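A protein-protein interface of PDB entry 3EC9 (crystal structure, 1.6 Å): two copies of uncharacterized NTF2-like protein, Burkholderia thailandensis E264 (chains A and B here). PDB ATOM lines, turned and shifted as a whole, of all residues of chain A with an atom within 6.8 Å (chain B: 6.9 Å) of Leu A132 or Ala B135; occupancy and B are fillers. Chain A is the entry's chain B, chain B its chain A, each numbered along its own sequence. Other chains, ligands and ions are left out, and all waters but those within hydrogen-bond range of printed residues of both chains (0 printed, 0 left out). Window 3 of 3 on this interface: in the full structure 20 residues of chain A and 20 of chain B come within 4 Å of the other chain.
N of Gly B48 is in hydrogen-bond range of OD2 of Asp A130, at 2.8 Å.
The backbone NH of Leu B132 is in hydrogen-bond range of the side-chain hydroxyl of Thr A131 (2.9 Å).
O of Thr B129 sits close to O of Thr A129.
The side-chain hydroxyl (OG1) of Thr B131 sits at hydrogen-bond distance from the backbone NH (N) of Thr A131 (3.2 Å).
OD1 of Asp A130 is in hydrogen-bond range of OG1 of Thr B131 (2.5 Å).
The backbone NH of Leu A132 sits at hydrogen-bond distance from the side-chain hydroxyl of Thr B131.
The side-chain carboxylate (OD2) of Asp B130 lies within hydrogen-bond range of the backbone NH (N) of Gly A48 (2.9 Å).
The side-chain hydroxyl of Thr A131 sits at hydrogen-bond distance from the side-chain carboxylate of Asp B130, 2.6 Å away.
The backbone NH (N) of Leu A132 lies close to the backbone NH (N) of Leu B132, at 3.5 Å.
Among the printed residues, merely in contact across the chains: Asp A130 with Ala B47, Leu A132 with Gly B48, Gly A48 with Leu B132, Leu A133 with Gly B48, Gly A48 with Leu B133, Leu A132 with Ala B135 and Leu A133 with Ala B47.
Of chain B, only Gly B48 (3.4 Å), Thr B131 (2.9 Å), Leu B132 (3.5 Å) and Ala B135 (3.9 Å) come within 4 Å of Leu A132.
Printed residues of chain A within 4 Å of Ala B135: Leu A132.
Printed residues of chain B within 4 Å of Leu A133: Ala B47 (3.9 Å) and Gly B48 (3.6 Å).
Of the printed residues of chain A, Ala B47 touches Asp A130 (3.4 Å) and Leu A133 (3.9 Å).
Of the printed residues of chain A, Asp B130 touches Gly A48 and Thr A131.
Printed residues of chain A within 4 Å of Leu B133: Gly A48 (3.7 Å).
Ala B137 touches none of the printed residues of chain A.
The nearest residue of chain B that does not touch Leu A132 is Phe B49 (5.5 Å).
Of the 10 printed residues of chain A, 6 touch a printed residue of chain B.
Hydrophobic or aromatic side chains of chain A within 4 Å of the printed part of chain B: Leu A132 and Leu A133.
Of the 18 printed residues of chain B, 8 touch a printed residue of chain A.
Hydrophobic or aromatic side chains of chain B that line the printed part of chain A: Ala B47, Leu B132, Leu B133 and Ala B135.
Among the printed residues, 16 pairs touch across the chains.
Gly A48 touches Leu B132, and with the chains exchanged Leu A132 touches Gly B48.
Thr B129 touches its own counterpart, Thr A129.
Asp A130 touches Thr B131, and with the chains exchanged Thr A131 touches Asp B130.
Thr A131 touches its own counterpart, Thr B131.
Positions printed for both chains: 48, 129, 130, 131, 132, 133, 134, 135, 136 and 137.
Of the 16 pairs that touch across the chains among the printed residues, 13 have their exchanged pair printed and touching as well.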
ATOM      1  N   GLY A  48      11.322   0.685  -7.907  1.00  0.00           N
ATOM      2  CA  GLY A  48      11.539   1.230  -6.554  1.00  0.00           C
ATOM      3  C   GLY A  48      10.359   1.895  -5.884  1.00  0.00           C
ATOM      4  O   GLY A  48      10.481   2.333  -4.737  1.00  0.00           O
ATOM      5  N   THR A 129       9.757   7.903 -11.485  1.00  0.00           N
ATOM      6  CA  THR A 129       9.698   8.870 -10.406  1.00  0.00           C
ATOM      7  C   THR A 129      10.837   8.728  -9.414  1.00  0.00           C
ATOM      8  O   THR A 129      11.630   7.770  -9.482  1.00  0.00           O
ATOM      9  CB  THR A 129       8.331   8.815  -9.701  1.00  0.00           C
ATOM     10  OG1 THR A 129       8.111   9.990  -8.887  1.00  0.00           O
ATOM     11  CG2 THR A 129       8.178   7.537  -8.872  1.00  0.00           C
ATOM     12  N   ASP A 130      10.914   9.688  -8.486  1.00  0.00           N
ATOM     13  CA  ASP A 130      12.029   9.766  -7.540  1.00  0.00           C
ATOM     14  C   ASP A 130      11.761   8.857  -6.392  1.00  0.00           C
ATOM     15  O   ASP A 130      11.314   9.230  -5.301  1.00  0.00           O
ATOM     16  CB  ASP A 130      12.220  11.231  -7.146  1.00  0.00           C
ATOM     17  CG  ASP A 130      13.640  11.540  -6.662  1.00  0.00           C
ATOM     18  OD1 ASP A 130      14.331  10.634  -6.135  1.00  0.00           O
ATOM     19  OD2 ASP A 130      14.067  12.721  -6.782  1.00  0.00           O
ATOM     20  N   THR A 131      12.010   7.590  -6.651  1.00  0.00           N
ATOM     21  CA  THR A 131      11.690   6.567  -5.671  1.00  0.00           C
ATOM     22  C   THR A 131      12.415   6.717  -4.329  1.00  0.00           C
ATOM     23  O   THR A 131      11.899   6.307  -3.279  1.00  0.00           O
ATOM     24  CB  THR A 131      11.923   5.181  -6.309  1.00  0.00           C
ATOM     25  OG1 THR A 131      13.228   5.160  -6.843  1.00  0.00           O
ATOM     26  CG2 THR A 131      10.901   4.913  -7.439  1.00  0.00           C
ATOM     27  N   LEU A 132      13.613   7.300  -4.341  1.00  0.00           N
ATOM     28  CA  LEU A 132      14.322   7.550  -3.078  1.00  0.00           C
ATOM     29  C   LEU A 132      13.537   8.562  -2.222  1.00  0.00           C
ATOM     30  O   LEU A 132      13.363   8.358  -1.036  1.00  0.00           O
ATOM     31  CB  LEU A 132      15.746   8.049  -3.317  1.00  0.00           C
ATOM     32  CG  LEU A 132      16.543   8.345  -2.059  1.00  0.00           C
ATOM     33  CD1 LEU A 132      16.757   7.036  -1.258  1.00  0.00           C
ATOM     34  CD2 LEU A 132      17.888   9.032  -2.377  1.00  0.00           C
ATOM     35  N   LEU A 133      13.086   9.649  -2.819  1.00  0.00           N
ATOM     36  CA  LEU A 133      12.304  10.641  -2.032  1.00  0.00           C
ATOM     37  C   LEU A 133      11.005  10.076  -1.496  1.00  0.00           C
ATOM     38  O   LEU A 133      10.603  10.412  -0.389  1.00  0.00           O
ATOM     39  CB  LEU A 133      12.064  11.922  -2.830  1.00  0.00           C
ATOM     40  CG  LEU A 133      13.202  12.963  -2.798  1.00  0.00           C
ATOM     41  CD1 LEU A 133      14.588  12.432  -3.164  1.00  0.00           C
ATOM     42  CD2 LEU A 133      12.861  14.226  -3.630  1.00  0.00           C
ATOM     43  N   VAL A 134      10.313   9.243  -2.276  1.00  0.00           N
ATOM     44  CA  VAL A 134       9.118   8.583  -1.762  1.00  0.00           C
ATOM     45  C   VAL A 134       9.465   7.641  -0.585  1.00  0.00           C
ATOM     46  O   VAL A 134       8.852   7.653   0.493  1.00  0.00           O
ATOM     47  CB  VAL A 134       8.431   7.809  -2.896  1.00  0.00           C
ATOM     48  CG1 VAL A 134       7.215   7.052  -2.311  1.00  0.00           C
ATOM     49  CG2 VAL A 134       8.024   8.743  -4.067  1.00  0.00           C
ATOM     50  N   ALA A 135      10.509   6.856  -0.784  1.00  0.00           N
ATOM     51  CA  ALA A 135      11.023   5.958   0.247  1.00  0.00           C
ATOM     52  C   ALA A 135      11.429   6.693   1.550  1.00  0.00           C
ATOM     53  O   ALA A 135      11.217   6.178   2.655  1.00  0.00           O
ATOM     54  CB  ALA A 135      12.196   5.121  -0.321  1.00  0.00           C
ATOM     55  N   GLN A 136      11.990   7.881   1.444  1.00  0.00           N
ATOM     56  CA  GLN A 136      12.389   8.661   2.626  1.00  0.00           C
ATOM     57  C   GLN A 136      11.173   8.961   3.513  1.00  0.00           C
ATOM     58  O   GLN A 136      11.270   9.017   4.745  1.00  0.00           O
ATOM     59  CB  GLN A 136      13.069   9.973   2.215  1.00  0.00           C
ATOM     60  CG  GLN A 136      14.481   9.857   1.704  1.00  0.00           C
ATOM     61  CD  GLN A 136      15.014  11.170   1.030  1.00  0.00           C
ATOM     62  OE1 GLN A 136      14.288  12.155   0.824  1.00  0.00           O
ATOM     63  NE2 GLN A 136      16.285  11.170   0.725  1.00  0.00           N
ATOM     64  N   ALA A 137      10.032   9.218   2.889  1.00  0.00           N
ATOM     65  CA  ALA A 137       8.798   9.517   3.610  1.00  0.00           C
ATOM     66  C   ALA A 137       8.295   8.277   4.382  1.00  0.00           C
ATOM     67  O   ALA A 137       7.513   8.406   5.307  1.00  0.00           O
ATOM     68  CB  ALA A 137       7.725  10.034   2.654  1.00  0.00           C
ATOM     69  N   ALA B  47      16.469  14.899  -8.246  1.00  0.00           N
ATOM     70  CA  ALA B  47      16.754  15.230  -6.857  1.00  0.00           C
ATOM     71  C   ALA B  47      17.373  14.119  -6.043  1.00  0.00           C
ATOM     72  O   ALA B  47      18.324  14.341  -5.285  1.00  0.00           O
ATOM     73  CB  ALA B  47      15.465  15.745  -6.172  1.00  0.00           C
ATOM     74  N   GLY B  48      16.841  12.906  -6.192  1.00  0.00           N
ATOM     75  CA  GLY B  48      17.334  11.751  -5.413  1.00  0.00           C
ATOM     76  C   GLY B  48      18.569  11.032  -5.974  1.00  0.00           C
ATOM     77  O   GLY B  48      19.101  10.083  -5.365  1.00  0.00           O
ATOM     78  N   PHE B  49      19.018  11.485  -7.146  1.00  0.00           N
ATOM     79  CA  PHE B  49      20.178  10.930  -7.845  1.00  0.00           C
ATOM     80  C   PHE B  49      21.481  11.521  -7.273  1.00  0.00           C
ATOM     81  O   PHE B  49      21.459  12.671  -6.870  1.00  0.00           O
ATOM     82  CB  PHE B  49      20.056  11.216  -9.353  1.00  0.00           C
ATOM     83  CG  PHE B  49      20.984  10.397 -10.198  1.00  0.00           C
ATOM     84  CD1 PHE B  49      20.793   9.051 -10.413  1.00  0.00           C
ATOM     85  CD2 PHE B  49      22.088  11.014 -10.804  1.00  0.00           C
ATOM     86  CE1 PHE B  49      21.698   8.329 -11.167  1.00  0.00           C
ATOM     87  CE2 PHE B  49      23.007  10.301 -11.548  1.00  0.00           C
ATOM     88  CZ  PHE B  49      22.804   8.938 -11.757  1.00  0.00           C
ATOM     89  N   PRO B  50      22.556  10.737  -7.207  1.00  0.00           N
ATOM     90  CA  PRO B  50      23.747  11.329  -6.529  1.00  0.00           C
ATOM     91  C   PRO B  50      24.253  12.624  -7.152  1.00  0.00           C
ATOM     92  O   PRO B  50      24.723  13.511  -6.419  1.00  0.00           O
ATOM     93  CB  PRO B  50      24.825  10.229  -6.616  1.00  0.00           C
ATOM     94  CG  PRO B  50      24.220   9.131  -7.453  1.00  0.00           C
ATOM     95  CD  PRO B  50      22.727   9.312  -7.489  1.00  0.00           C
ATOM     96  N   TRP B  73      31.791   5.311 -10.021  1.00  0.00           N
ATOM     97  CA  TRP B  73      31.149   4.099 -10.550  1.00  0.00           C
ATOM     98  C   TRP B  73      32.086   3.439 -11.558  1.00  0.00           C
ATOM     99  O   TRP B  73      32.773   4.106 -12.314  1.00  0.00           O
ATOM    100  CB  TRP B  73      29.810   4.418 -11.249  1.00  0.00           C
ATOM    101  CG  TRP B  73      28.809   5.038 -10.351  1.00  0.00           C
ATOM    102  CD1 TRP B  73      28.704   6.340 -10.027  1.00  0.00           C
ATOM    103  CD2 TRP B  73      27.742   4.364  -9.655  1.00  0.00           C
ATOM    104  NE1 TRP B  73      27.679   6.540  -9.119  1.00  0.00           N
ATOM    105  CE2 TRP B  73      27.029   5.354  -8.917  1.00  0.00           C
ATOM    106  CE3 TRP B  73      27.324   3.027  -9.575  1.00  0.00           C
ATOM    107  CZ2 TRP B  73      25.948   5.031  -8.090  1.00  0.00           C
ATOM    108  CZ3 TRP B  73      26.231   2.728  -8.798  1.00  0.00           C
ATOM    109  CH2 TRP B  73      25.568   3.722  -8.048  1.00  0.00           C
ATOM    110  N   PHE B 107      23.774  -2.087  -9.774  1.00  0.00           N
ATOM    111  CA  PHE B 107      22.334  -1.888  -9.932  1.00  0.00           C
ATOM    112  C   PHE B 107      22.005  -1.898 -11.421  1.00  0.00           C
ATOM    113  O   PHE B 107      22.880  -1.775 -12.280  1.00  0.00           O
ATOM    114  CB  PHE B 107      21.904  -0.541  -9.340  1.00  0.00           C
ATOM    115  CG  PHE B 107      22.169   0.601 -10.267  1.00  0.00           C
ATOM    116  CD1 PHE B 107      23.415   1.192 -10.288  1.00  0.00           C
ATOM    117  CD2 PHE B 107      21.186   1.111 -11.060  1.00  0.00           C
ATOM    118  CE1 PHE B 107      23.703   2.226 -11.135  1.00  0.00           C
ATOM    119  CE2 PHE B 107      21.441   2.122 -11.909  1.00  0.00           C
ATOM    120  CZ  PHE B 107      22.697   2.696 -11.961  1.00  0.00           C
ATOM    121  N   THR B 129      14.665   8.815 -12.999  1.00  0.00           N
ATOM    122  CA  THR B 129      15.214   7.480 -12.806  1.00  0.00           C
ATOM    123  C   THR B 129      14.911   6.930 -11.425  1.00  0.00           C
ATOM    124  O   THR B 129      14.416   7.656 -10.543  1.00  0.00           O
ATOM    125  CB  THR B 129      16.727   7.436 -13.116  1.00  0.00           C
ATOM    126  OG1 THR B 129      17.169   6.058 -13.269  1.00  0.00           O
ATOM    127  CG2 THR B 129      17.559   8.113 -12.026  1.00  0.00           C
ATOM    128  N   ASP B 130      15.210   5.637 -11.245  1.00  0.00           N
ATOM    129  CA  ASP B 130      14.854   4.889 -10.014  1.00  0.00           C
ATOM    130  C   ASP B 130      15.925   5.168  -8.973  1.00  0.00           C
ATOM    131  O   ASP B 130      16.874   4.384  -8.720  1.00  0.00           O
ATOM    132  CB  ASP B 130      14.726   3.406 -10.362  1.00  0.00           C
ATOM    133  CG  ASP B 130      13.819   2.648  -9.402  1.00  0.00           C
ATOM    134  OD1 ASP B 130      13.802   2.982  -8.202  1.00  0.00           O
ATOM    135  OD2 ASP B 130      13.168   1.661  -9.862  1.00  0.00           O
ATOM    136  N   THR B 131      15.809   6.348  -8.372  1.00  0.00           N
ATOM    137  CA  THR B 131      16.823   6.799  -7.432  1.00  0.00           C
ATOM    138  C   THR B 131      16.992   5.891  -6.215  1.00  0.00           C
ATOM    139  O   THR B 131      18.080   5.822  -5.658  1.00  0.00           O
ATOM    140  CB  THR B 131      16.499   8.220  -7.019  1.00  0.00           C
ATOM    141  OG1 THR B 131      15.122   8.279  -6.621  1.00  0.00           O
ATOM    142  CG2 THR B 131      16.796   9.204  -8.171  1.00  0.00           C
ATOM    143  N   LEU B 132      15.938   5.184  -5.822  1.00  0.00           N
ATOM    144  CA  LEU B 132      16.061   4.174  -4.742  1.00  0.00           C
ATOM    145  C   LEU B 132      16.990   3.019  -5.130  1.00  0.00           C
ATOM    146  O   LEU B 132      17.856   2.627  -4.331  1.00  0.00           O
ATOM    147  CB  LEU B 132      14.713   3.611  -4.325  1.00  0.00           C
ATOM    148  CG  LEU B 132      14.805   2.625  -3.171  1.00  0.00           C
ATOM    149  CD1 LEU B 132      15.422   3.248  -1.886  1.00  0.00           C
ATOM    150  CD2 LEU B 132      13.428   1.955  -2.891  1.00  0.00           C
ATOM    151  N   LEU B 133      16.782   2.467  -6.326  1.00  0.00           N
ATOM    152  CA  LEU B 133      17.660   1.395  -6.798  1.00  0.00           C
ATOM    153  C   LEU B 133      19.117   1.833  -6.903  1.00  0.00           C
ATOM    154  O   LEU B 133      20.015   1.054  -6.567  1.00  0.00           O
ATOM    155  CB  LEU B 133      17.181   0.767  -8.081  1.00  0.00           C
ATOM    156  CG  LEU B 133      16.162  -0.409  -7.962  1.00  0.00           C
ATOM    157  CD1 LEU B 133      14.934  -0.114  -7.091  1.00  0.00           C
ATOM    158  CD2 LEU B 133      15.717  -0.913  -9.306  1.00  0.00           C
ATOM    159  N   VAL B 134      19.360   3.058  -7.376  1.00  0.00           N
ATOM    160  CA  VAL B 134      20.741   3.578  -7.419  1.00  0.00           C
ATOM    161  C   VAL B 134      21.324   3.729  -5.983  1.00  0.00           C
ATOM    162  O   VAL B 134      22.465   3.288  -5.669  1.00  0.00           O
ATOM    163  CB  VAL B 134      20.756   4.910  -8.156  1.00  0.00           C
ATOM    164  CG1 VAL B 134      22.143   5.574  -8.073  1.00  0.00           C
ATOM    165  CG2 VAL B 134      20.314   4.758  -9.616  1.00  0.00           C
ATOM    166  N   ALA B 135      20.525   4.296  -5.096  1.00  0.00           N
ATOM    167  CA  ALA B 135      20.899   4.509  -3.681  1.00  0.00           C
ATOM    168  C   ALA B 135      21.243   3.200  -2.955  1.00  0.00           C
ATOM    169  O   ALA B 135      22.167   3.134  -2.128  1.00  0.00           O
ATOM    170  CB  ALA B 135      19.765   5.228  -2.943  1.00  0.00           C
ATOM    171  N   GLN B 136      20.521   2.137  -3.302  1.00  0.00           N
ATOM    172  CA  GLN B 136      20.746   0.797  -2.709  1.00  0.00           C
ATOM    173  C   GLN B 136      22.164   0.284  -2.980  1.00  0.00           C
ATOM    174  O   GLN B 136      22.790  -0.345  -2.115  1.00  0.00           O
ATOM    175  CB  GLN B 136      19.707  -0.190  -3.254  1.00  0.00           C
ATOM    176  CG  GLN B 136      18.361  -0.196  -2.544  1.00  0.00           C
ATOM    177  CD  GLN B 136      17.263  -0.995  -3.324  1.00  0.00           C
ATOM    178  OE1 GLN B 136      17.516  -1.585  -4.390  1.00  0.00           O
ATOM    179  NE2 GLN B 136      16.075  -1.018  -2.771  1.00  0.00           N
ATOM    180  N   ALA B 137      22.665   0.527  -4.191  1.00  0.00           N
ATOM    181  CA  ALA B 137      24.032   0.128  -4.610  1.00  0.00           C
ATOM    182  C   ALA B 137      25.106   0.881  -3.794  1.00  0.00           C
ATOM    183  O   ALA B 137      26.238   0.438  -3.695  1.00  0.00           O
ATOM    184  CB  ALA B 137      24.206   0.411  -6.120  1.00  0.00           C
ATOM    185  N   MET B 138      24.738   2.042  -3.246  1.00  0.00           N
ATOM    186  CA  MET B 138      25.690   2.919  -2.543  1.00  0.00           C
ATOM    187  C   MET B 138      25.728   2.608  -1.053  1.00  0.00           C
ATOM    188  O   MET B 138      26.651   3.033  -0.352  1.00  0.00           O
ATOM    189  CB  MET B 138      25.331   4.389  -2.772  1.00  0.00           C
ATOM    190  CG  MET B 138      25.354   4.807  -4.255  1.00  0.00           C
ATOM    191  SD  MET B 138      25.272   6.756  -4.622  1.00  0.00           S
ATOM    192  CE  MET B 138      23.480   7.111  -3.928  1.00  0.00           C
ATOM    193  N   GLN B 139      24.748   1.847  -0.578  1.00  0.00           N
ATOM    194  CA  GLN B 139      24.711   1.457   0.843  1.00  0.00           C
ATOM    195  C   GLN B 139      25.802   0.447   1.175  1.00  0.00           C
ATOM    196  O   GLN B 139      25.959  -0.552   0.475  1.00  0.00           O
ATOM    197  CB  GLN B 139      23.358   0.860   1.213  1.00  0.00           C
ATOM    198  CG  GLN B 139      22.246   1.885   1.277  1.00  0.00           C
ATOM    199  CD  GLN B 139      20.857   1.275   1.251  1.00  0.00           C
ATOM    200  OE1 GLN B 139      19.902   1.914   0.807  1.00  0.00           O
ATOM    201  NE2 GLN B 139      20.739   0.041   1.711  1.00  0.00           N
ATOM    202  N   PRO B 140      26.564   0.704   2.249  1.00  0.00           N
ATOM    203  CA  PRO B 140      27.506  -0.278   2.756  1.00  0.00           C
ATOM    204  C   PRO B 140      26.845  -1.612   3.128  1.00  0.00           C
ATOM    205  O   PRO B 140      27.545  -2.624   3.136  1.00  0.00           O
ATOM    206  CB  PRO B 140      28.074   0.391   4.008  1.00  0.00           C
ATOM    207  CG  PRO B 140      27.865   1.831   3.806  1.00  0.00           C
ATOM    208  CD  PRO B 140      26.622   1.965   3.017  1.00  0.00           C
ATOM    209  OXT PRO B 140      25.630  -1.733   3.394  1.00  0.00           O
